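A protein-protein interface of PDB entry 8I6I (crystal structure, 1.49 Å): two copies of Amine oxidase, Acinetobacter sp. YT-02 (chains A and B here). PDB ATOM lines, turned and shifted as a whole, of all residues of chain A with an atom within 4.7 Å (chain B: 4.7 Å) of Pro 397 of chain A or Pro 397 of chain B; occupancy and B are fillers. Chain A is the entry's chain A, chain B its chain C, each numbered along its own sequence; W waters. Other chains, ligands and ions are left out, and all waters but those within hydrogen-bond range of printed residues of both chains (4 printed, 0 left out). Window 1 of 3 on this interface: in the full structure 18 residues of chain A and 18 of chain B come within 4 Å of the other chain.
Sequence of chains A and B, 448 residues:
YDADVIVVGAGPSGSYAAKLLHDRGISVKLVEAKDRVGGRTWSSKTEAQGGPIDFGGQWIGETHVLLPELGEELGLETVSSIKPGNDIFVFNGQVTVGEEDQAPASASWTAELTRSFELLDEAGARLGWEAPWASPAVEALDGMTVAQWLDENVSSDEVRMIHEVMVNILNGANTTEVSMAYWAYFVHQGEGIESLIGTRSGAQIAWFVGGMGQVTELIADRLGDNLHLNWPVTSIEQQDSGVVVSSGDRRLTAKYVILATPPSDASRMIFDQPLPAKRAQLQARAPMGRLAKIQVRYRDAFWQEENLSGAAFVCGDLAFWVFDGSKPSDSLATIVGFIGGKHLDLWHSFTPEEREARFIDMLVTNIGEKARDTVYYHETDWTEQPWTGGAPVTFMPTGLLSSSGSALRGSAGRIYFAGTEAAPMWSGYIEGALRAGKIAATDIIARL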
ATOM      1  N   ASP A 142      17.475   5.464  10.919  1.00  0.00           N
ATOM      2  CA  ASP A 142      16.274   4.739  11.394  1.00  0.00           C
ATOM      3  C   ASP A 142      16.316   4.492  12.888  1.00  0.00           C
ATOM      4  O   ASP A 142      15.303   4.062  13.448  1.00  0.00           O
ATOM      5  CB  ASP A 142      16.082   3.423  10.669  1.00  0.00           C
ATOM      6  CG  ASP A 142      14.644   2.959  10.673  1.00  0.00           C
ATOM      7  OD1 ASP A 142      13.749   3.833  10.611  1.00  0.00           O
ATOM      8  OD2 ASP A 142      14.431   1.737  10.644  1.00  0.00           O
ATOM      9  N   GLU A 177       8.161  11.013  17.613  1.00  0.00           N
ATOM     10  CA  GLU A 177       7.495   9.715  17.315  1.00  0.00           C
ATOM     11  C   GLU A 177       7.966   9.099  16.006  1.00  0.00           C
ATOM     12  O   GLU A 177       7.863   7.862  15.833  1.00  0.00           O
ATOM     13  CB  GLU A 177       5.982   9.911  17.274  1.00  0.00           C
ATOM     14  CG  GLU A 177       5.391  10.325  18.598  1.00  0.00           C
ATOM     15  CD  GLU A 177       3.977  10.903  18.532  1.00  0.00           C
ATOM     16  OE1 GLU A 177       3.429  11.081  19.650  1.00  0.00           O
ATOM     17  OE2 GLU A 177       3.412  11.053  17.424  1.00  0.00           O
ATOM     18  N   SER A 179      10.543   8.063  12.951  1.00  0.00           N
ATOM     19  CA  SER A 179      11.926   7.766  12.568  1.00  0.00           C
ATOM     20  C   SER A 179      12.439   8.844  11.605  1.00  0.00           C
ATOM     21  O   SER A 179      11.750   9.182  10.618  1.00  0.00           O
ATOM     22  CB  SER A 179      11.961   6.460  11.888  1.00  0.00           C
ATOM     23  OG  SER A 179      13.097   6.294  11.071  1.00  0.00           O
ATOM     24  N   ARG A 285       3.176  -2.446  12.988  1.00  0.00           N
ATOM     25  CA  ARG A 285       4.063  -1.443  13.591  1.00  0.00           C
ATOM     26  C   ARG A 285       4.100  -0.127  12.821  1.00  0.00           C
ATOM     27  O   ARG A 285       4.780   0.776  13.326  1.00  0.00           O
ATOM     28  CB  ARG A 285       5.453  -2.045  13.840  1.00  0.00           C
ATOM     29  CG  ARG A 285       5.398  -3.062  14.988  1.00  0.00           C
ATOM     30  CD  ARG A 285       6.607  -3.958  15.106  1.00  0.00           C
ATOM     31  NE  ARG A 285       7.883  -3.237  15.086  1.00  0.00           N
ATOM     32  CZ  ARG A 285       8.999  -3.709  14.560  1.00  0.00           C
ATOM     33  NH1 ARG A 285      10.055  -2.901  14.534  1.00  0.00           N
ATOM     34  NH2 ARG A 285       9.108  -4.932  14.113  1.00  0.00           N
ATOM     35  N   PRO A 287       1.908   2.718  12.075  1.00  0.00           N
ATOM     36  CA  PRO A 287       0.599   3.261  12.374  1.00  0.00           C
ATOM     37  C   PRO A 287       0.259   4.432  11.468  1.00  0.00           C
ATOM     38  O   PRO A 287       1.061   4.942  10.725  1.00  0.00           O
ATOM     39  CB  PRO A 287       0.693   3.783  13.808  1.00  0.00           C
ATOM     40  CG  PRO A 287       2.134   3.885  14.099  1.00  0.00           C
ATOM     41  CD  PRO A 287       2.932   3.209  13.000  1.00  0.00           C
ATOM     42  N   PHE A 395       2.913   6.443   9.079  1.00  0.00           N
ATOM     43  CA  PHE A 395       4.283   6.799   9.480  1.00  0.00           C
ATOM     44  C   PHE A 395       4.955   5.567  10.093  1.00  0.00           C
ATOM     45  O   PHE A 395       4.323   4.547  10.313  1.00  0.00           O
ATOM     46  CB  PHE A 395       4.364   8.015  10.392  1.00  0.00           C
ATOM     47  CG  PHE A 395       3.939   7.798  11.823  1.00  0.00           C
ATOM     48  CD1 PHE A 395       2.624   7.914  12.217  1.00  0.00           C
ATOM     49  CD2 PHE A 395       4.884   7.468  12.777  1.00  0.00           C
ATOM     50  CE1 PHE A 395       2.235   7.658  13.514  1.00  0.00           C
ATOM     51  CE2 PHE A 395       4.510   7.296  14.099  1.00  0.00           C
ATOM     52  CZ  PHE A 395       3.185   7.377  14.462  1.00  0.00           C
ATOM     53  N   MET A 396       6.261   5.675  10.328  1.00  0.00           N
ATOM     54  CA  MET A 396       6.985   4.572  10.998  1.00  0.00           C
ATOM     55  C   MET A 396       7.807   5.135  12.148  1.00  0.00           C
ATOM     56  O   MET A 396       8.440   6.204  11.990  1.00  0.00           O
ATOM     57  CB  MET A 396       7.898   3.831  10.045  1.00  0.00           C
ATOM     58  CG  MET A 396       7.148   3.238   8.913  1.00  0.00           C
ATOM     59  SD  MET A 396       8.234   2.210   7.913  1.00  0.00           S
ATOM     60  CE  MET A 396       7.149   1.811   6.545  1.00  0.00           C
ATOM     61  N   PRO A 397       7.799   4.442  13.290  1.00  0.00           N
ATOM     62  CA  PRO A 397       8.720   4.700  14.381  1.00  0.00           C
ATOM     63  C   PRO A 397      10.113   4.121  14.098  1.00  0.00           C
ATOM     64  O   PRO A 397      10.344   3.477  13.090  1.00  0.00           O
ATOM     65  CB  PRO A 397       8.084   3.968  15.548  1.00  0.00           C
ATOM     66  CG  PRO A 397       7.480   2.757  14.891  1.00  0.00           C
ATOM     67  CD  PRO A 397       7.016   3.226  13.520  1.00  0.00           C
ATOM     68  N   THR A 398      10.995   4.358  15.049  1.00  0.00           N
ATOM     69  CA  THR A 398      12.384   3.887  14.898  1.00  0.00           C
ATOM     70  C   THR A 398      12.441   2.375  14.674  1.00  0.00           C
ATOM     71  O   THR A 398      11.690   1.576  15.282  1.00  0.00           O
ATOM     72  CB  THR A 398      13.247   4.320  16.082  1.00  0.00           C
ATOM     73  OG1 THR A 398      12.747   3.802  17.317  1.00  0.00           O
ATOM     74  CG2 THR A 398      13.478   5.805  16.165  1.00  0.00           C
ATOM     75  N   GLY A 399      13.347   1.971  13.799  1.00  0.00           N
ATOM     76  CA  GLY A 399      13.675   0.558  13.591  1.00  0.00           C
ATOM     77  C   GLY A 399      12.910  -0.122  12.476  1.00  0.00           C
ATOM     78  O   GLY A 399      13.383  -1.188  12.007  1.00  0.00           O
ATOM     79  N   LEU A 400      11.757   0.375  12.039  1.00  0.00           N
ATOM     80  CA  LEU A 400      10.834  -0.405  11.185  1.00  0.00           C
ATOM     81  C   LEU A 400      11.270  -0.305   9.737  1.00  0.00           C
ATOM     82  O   LEU A 400      11.338  -1.360   9.077  1.00  0.00           O
ATOM     83  CB  LEU A 400       9.387   0.060  11.354  1.00  0.00           C
ATOM     84  CG  LEU A 400       8.349  -0.834  10.678  1.00  0.00           C
ATOM     85  CD1 LEU A 400       8.353  -2.245  11.236  1.00  0.00           C
ATOM     86  CD2 LEU A 400       6.964  -0.233  10.828  1.00  0.00           C
ATOM     87  N   ASP B 142      11.381   9.391  27.214  1.00  0.00           N
ATOM     88  CA  ASP B 142      10.456   8.793  26.233  1.00  0.00           C
ATOM     89  C   ASP B 142      10.772   9.260  24.831  1.00  0.00           C
ATOM     90  O   ASP B 142      10.136   8.775  23.921  1.00  0.00           O
ATOM     91  CB  ASP B 142       9.025   9.175  26.607  1.00  0.00           C
ATOM     92  CG  ASP B 142       7.989   8.275  25.994  1.00  0.00           C
ATOM     93  OD1 ASP B 142       8.302   7.073  25.855  1.00  0.00           O
ATOM     94  OD2 ASP B 142       6.900   8.748  25.668  1.00  0.00           O
ATOM     95  N   GLU B 177      14.026   0.016  18.916  1.00  0.00           N
ATOM     96  CA  GLU B 177      12.569   0.112  18.699  1.00  0.00           C
ATOM     97  C   GLU B 177      11.840   0.593  19.935  1.00  0.00           C
ATOM     98  O   GLU B 177      10.714   1.051  19.781  1.00  0.00           O
ATOM     99  CB  GLU B 177      12.038  -1.251  18.249  1.00  0.00           C
ATOM    100  CG  GLU B 177      12.555  -1.670  16.885  1.00  0.00           C
ATOM    101  CD  GLU B 177      12.407  -3.139  16.519  1.00  0.00           C
ATOM    102  OE1 GLU B 177      12.654  -3.460  15.319  1.00  0.00           O
ATOM    103  OE2 GLU B 177      11.964  -3.957  17.376  1.00  0.00           O
ATOM    104  N   SER B 179      11.082   2.612  23.448  1.00  0.00           N
ATOM    105  CA  SER B 179      11.328   3.841  24.216  1.00  0.00           C
ATOM    106  C   SER B 179      12.141   3.479  25.471  1.00  0.00           C
ATOM    107  O   SER B 179      11.734   2.541  26.207  1.00  0.00           O
ATOM    108  CB  SER B 179      10.019   4.412  24.653  1.00  0.00           C
ATOM    109  OG  SER B 179      10.192   5.326  25.706  1.00  0.00           O
ATOM    110  N   ARG B 285      -0.751   2.115  18.684  1.00  0.00           N
ATOM    111  CA  ARG B 285       0.693   2.453  18.638  1.00  0.00           C
ATOM    112  C   ARG B 285       1.488   1.645  19.637  1.00  0.00           C
ATOM    113  O   ARG B 285       2.713   1.833  19.612  1.00  0.00           O
ATOM    114  CB  ARG B 285       0.905   3.971  18.766  1.00  0.00           C
ATOM    115  CG  ARG B 285       0.464   4.693  17.489  1.00  0.00           C
ATOM    116  CD  ARG B 285       0.333   6.211  17.682  1.00  0.00           C
ATOM    117  NE  ARG B 285       1.471   6.877  18.316  1.00  0.00           N
ATOM    118  CZ  ARG B 285       1.362   7.981  19.053  1.00  0.00           C
ATOM    119  NH1 ARG B 285       2.441   8.479  19.636  1.00  0.00           N
ATOM    120  NH2 ARG B 285       0.216   8.585  19.240  1.00  0.00           N
ATOM    121  N   PRO B 287       2.590  -1.852  20.075  1.00  0.00           N
ATOM    122  CA  PRO B 287       2.568  -3.165  19.450  1.00  0.00           C
ATOM    123  C   PRO B 287       3.059  -4.240  20.411  1.00  0.00           C
ATOM    124  O   PRO B 287       3.575  -3.959  21.514  1.00  0.00           O
ATOM    125  CB  PRO B 287       3.512  -3.027  18.259  1.00  0.00           C
ATOM    126  CG  PRO B 287       4.495  -1.988  18.696  1.00  0.00           C
ATOM    127  CD  PRO B 287       3.790  -1.096  19.689  1.00  0.00           C
ATOM    128  N   PHE B 395       5.033  -3.616  23.901  1.00  0.00           N
ATOM    129  CA  PHE B 395       6.063  -2.578  24.153  1.00  0.00           C
ATOM    130  C   PHE B 395       5.550  -1.257  23.571  1.00  0.00           C
ATOM    131  O   PHE B 395       4.523  -1.208  22.866  1.00  0.00           O
ATOM    132  CB  PHE B 395       7.428  -2.974  23.600  1.00  0.00           C
ATOM    133  CG  PHE B 395       7.597  -2.916  22.119  1.00  0.00           C
ATOM    134  CD1 PHE B 395       7.213  -3.998  21.346  1.00  0.00           C
ATOM    135  CD2 PHE B 395       8.101  -1.782  21.497  1.00  0.00           C
ATOM    136  CE1 PHE B 395       7.391  -3.993  19.986  1.00  0.00           C
ATOM    137  CE2 PHE B 395       8.235  -1.759  20.126  1.00  0.00           C
ATOM    138  CZ  PHE B 395       7.864  -2.841  19.359  1.00  0.00           C
ATOM    139  N   MET B 396       6.273  -0.180  23.823  1.00  0.00           N
ATOM    140  CA  MET B 396       5.957   1.156  23.284  1.00  0.00           C
ATOM    141  C   MET B 396       7.172   1.796  22.665  1.00  0.00           C
ATOM    142  O   MET B 396       8.252   1.723  23.218  1.00  0.00           O
ATOM    143  CB  MET B 396       5.424   2.097  24.333  1.00  0.00           C
ATOM    144  CG  MET B 396       4.201   1.584  24.992  1.00  0.00           C
ATOM    145  SD  MET B 396       3.484   2.826  26.065  1.00  0.00           S
ATOM    146  CE  MET B 396       2.254   1.888  26.948  1.00  0.00           C
ATOM    147  N   PRO B 397       7.007   2.425  21.490  1.00  0.00           N
ATOM    148  CA  PRO B 397       8.061   3.226  20.879  1.00  0.00           C
ATOM    149  C   PRO B 397       8.087   4.622  21.463  1.00  0.00           C
ATOM    150  O   PRO B 397       7.298   4.980  22.309  1.00  0.00           O
ATOM    151  CB  PRO B 397       7.622   3.281  19.418  1.00  0.00           C
ATOM    152  CG  PRO B 397       6.148   3.326  19.540  1.00  0.00           C
ATOM    153  CD  PRO B 397       5.778   2.451  20.712  1.00  0.00           C
ATOM    154  N   THR B 398       9.057   5.414  21.016  1.00  0.00           N
ATOM    155  CA  THR B 398       9.196   6.784  21.519  1.00  0.00           C
ATOM    156  C   THR B 398       7.895   7.583  21.395  1.00  0.00           C
ATOM    157  O   THR B 398       7.111   7.446  20.407  1.00  0.00           O
ATOM    158  CB  THR B 398      10.348   7.493  20.839  1.00  0.00           C
ATOM    159  OG1 THR B 398      10.114   7.582  19.436  1.00  0.00           O
ATOM    160  CG2 THR B 398      11.680   6.820  21.123  1.00  0.00           C
ATOM    161  N   GLY B 399       7.650   8.362  22.448  1.00  0.00           N
ATOM    162  CA  GLY B 399       6.559   9.324  22.510  1.00  0.00           C
ATOM    163  C   GLY B 399       5.237   8.805  23.064  1.00  0.00           C
ATOM    164  O   GLY B 399       4.397   9.651  23.444  1.00  0.00           O
ATOM    165  N   LEU B 400       5.028   7.506  23.178  1.00  0.00           N
ATOM    166  CA  LEU B 400       3.685   6.986  23.494  1.00  0.00           C
ATOM    167  C   LEU B 400       3.403   6.997  24.989  1.00  0.00           C
ATOM    168  O   LEU B 400       2.308   7.429  25.384  1.00  0.00           O
ATOM    169  CB  LEU B 400       3.514   5.601  22.856  1.00  0.00           C
ATOM    170  CG  LEU B 400       2.077   5.073  22.927  1.00  0.00           C
ATOM    171  CD1 LEU B 400       1.102   5.983  22.192  1.00  0.00           C
ATOM    172  CD2 LEU B 400       1.993   3.660  22.398  1.00  0.00           C
HETATM  173  O   HOH W   1      10.111   6.330  16.996  1.00  0.00           O
HETATM  174  O   HOH W   2      10.897   4.037  19.322  1.00  0.00           O
HETATM  175  O   HOH W   3       6.633   6.434  17.893  1.00  0.00           O
HETATM  176  O   HOH W   4       9.623   1.248  17.157  1.00  0.00           O
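Glu 177 of chain A touches Thr 398 of chain B. CG of Arg 285 of chain A touches CB of Pro 287 of chain B (3.8 Å). CB of Pro 287 of chain A touches CG of Arg 285 of chain B (3.8 Å). Pro 397 of chain B touches Pro 397 of chain A. Thr 398 of chain A touches Glu 177 of chain B.
Asp 142 of chain A touches none of the printed residues of chain B. Of the printed residues of chain B, Arg 285 of chain A touches Glu 177 (2.8 Å) and Pro 287 (3.8 Å). Printed residues of chain B within 4 Å of Pro 287 of chain A: Arg 285 (3.8 Å). Of chain B, only Pro 397 comes within 4 Å of Pro 397 of chain A. Of the printed residues of chain A, Pro 287 of chain B touches Arg 285. Pro 397 of chain B touches just one residue of chain A: Pro 397 (3.96 Å). The nearest printed residue of chain B that does not touch Pro 397 of chain A is Thr 398 of chain B (5.7 Å). The nearest printed residue of chain A that does not touch Thr 398 of chain B is Thr 398 of chain A (5.0 Å).
Glu 177 of chain A touches Arg 285 of chain B, and with the chains exchanged Arg 285 of chain A touches Glu 177 of chain B. Glu 177 of chain A touches Thr 398 of chain B, and with the chains exchanged Thr 398 of chain A touches Glu 177 of chain B. Arg 285 of chain A touches Pro 287 of chain B, and with the chains exchanged Pro 287 of chain A touches Arg 285 of chain B. Pro 397 of chain B touches its own counterpart, Pro 397 of chain A. Positions printed for both chains: 142, 177, 179, 285, 287, 395, 396, 397, 398, 399 and 400. Of the 7 pairs that touch across the chains among the printed residues, 7 have their exchanged pair printed and touching as well.
The backbone NH of Phe 395 of chain A sits at hydrogen-bond distance from the backbone carbonyl oxygen of Pro 287 of chain A, at 2.9 Å. The backbone carbonyl oxygen of Pro 287 of chain B is in hydrogen-bond range of the backbone NH of Phe 395 of chain B (2.8 Å).
Water W2 lies within hydrogen-bond range of OG1 of Thr 398 of chain A, N of Thr 398 of chain B and O of Glu 177 of chain B. Water W1 lies within hydrogen-bond range of OG1 of Thr 398 of chain B (2.7 Å), N of Thr 398 of chain A (2.9 Å) and O of Glu 177 of chain A (3.0 Å). Water W3 lies within hydrogen-bond range of O of Thr 398 of chain B and O of Glu 177 of chain A. Water W4 bridges O of Thr 398 of chain A (2.8 Å) and O of Glu 177 of chain B (2.8 Å).
Of the 11 printed residues of chain B, 5 touch a printed residue of chain A. Hydrophobic or aromatic side chains of chain B within 4 Å of the printed part of chain A: Pro 287 and Pro 397. Hydrophobic or aromatic side chains of chain A within 4 Å of the printed part of chain B: Pro 287 and Pro 397. Among the printed residues, 7 pairs touch across the chains. Among the printed residues, Asp or Glu carboxylates within 4 Å of a Lys or Arg side-chain nitrogen of the other chain: Glu 177 of chain A with Arg 285 of chain B (2.8 Å) and Arg 285 of chain A with Glu 177 of chain B (2.8 Å).
The guanidinium group of Arg 285 of chain B lies within salt-bridge range of the side-chain carboxylate of Glu 177 of chain A. NH1 of Arg 285 of chain A is in salt-bridge range of OE1 of Glu 177 of chain B (2.8 Å).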
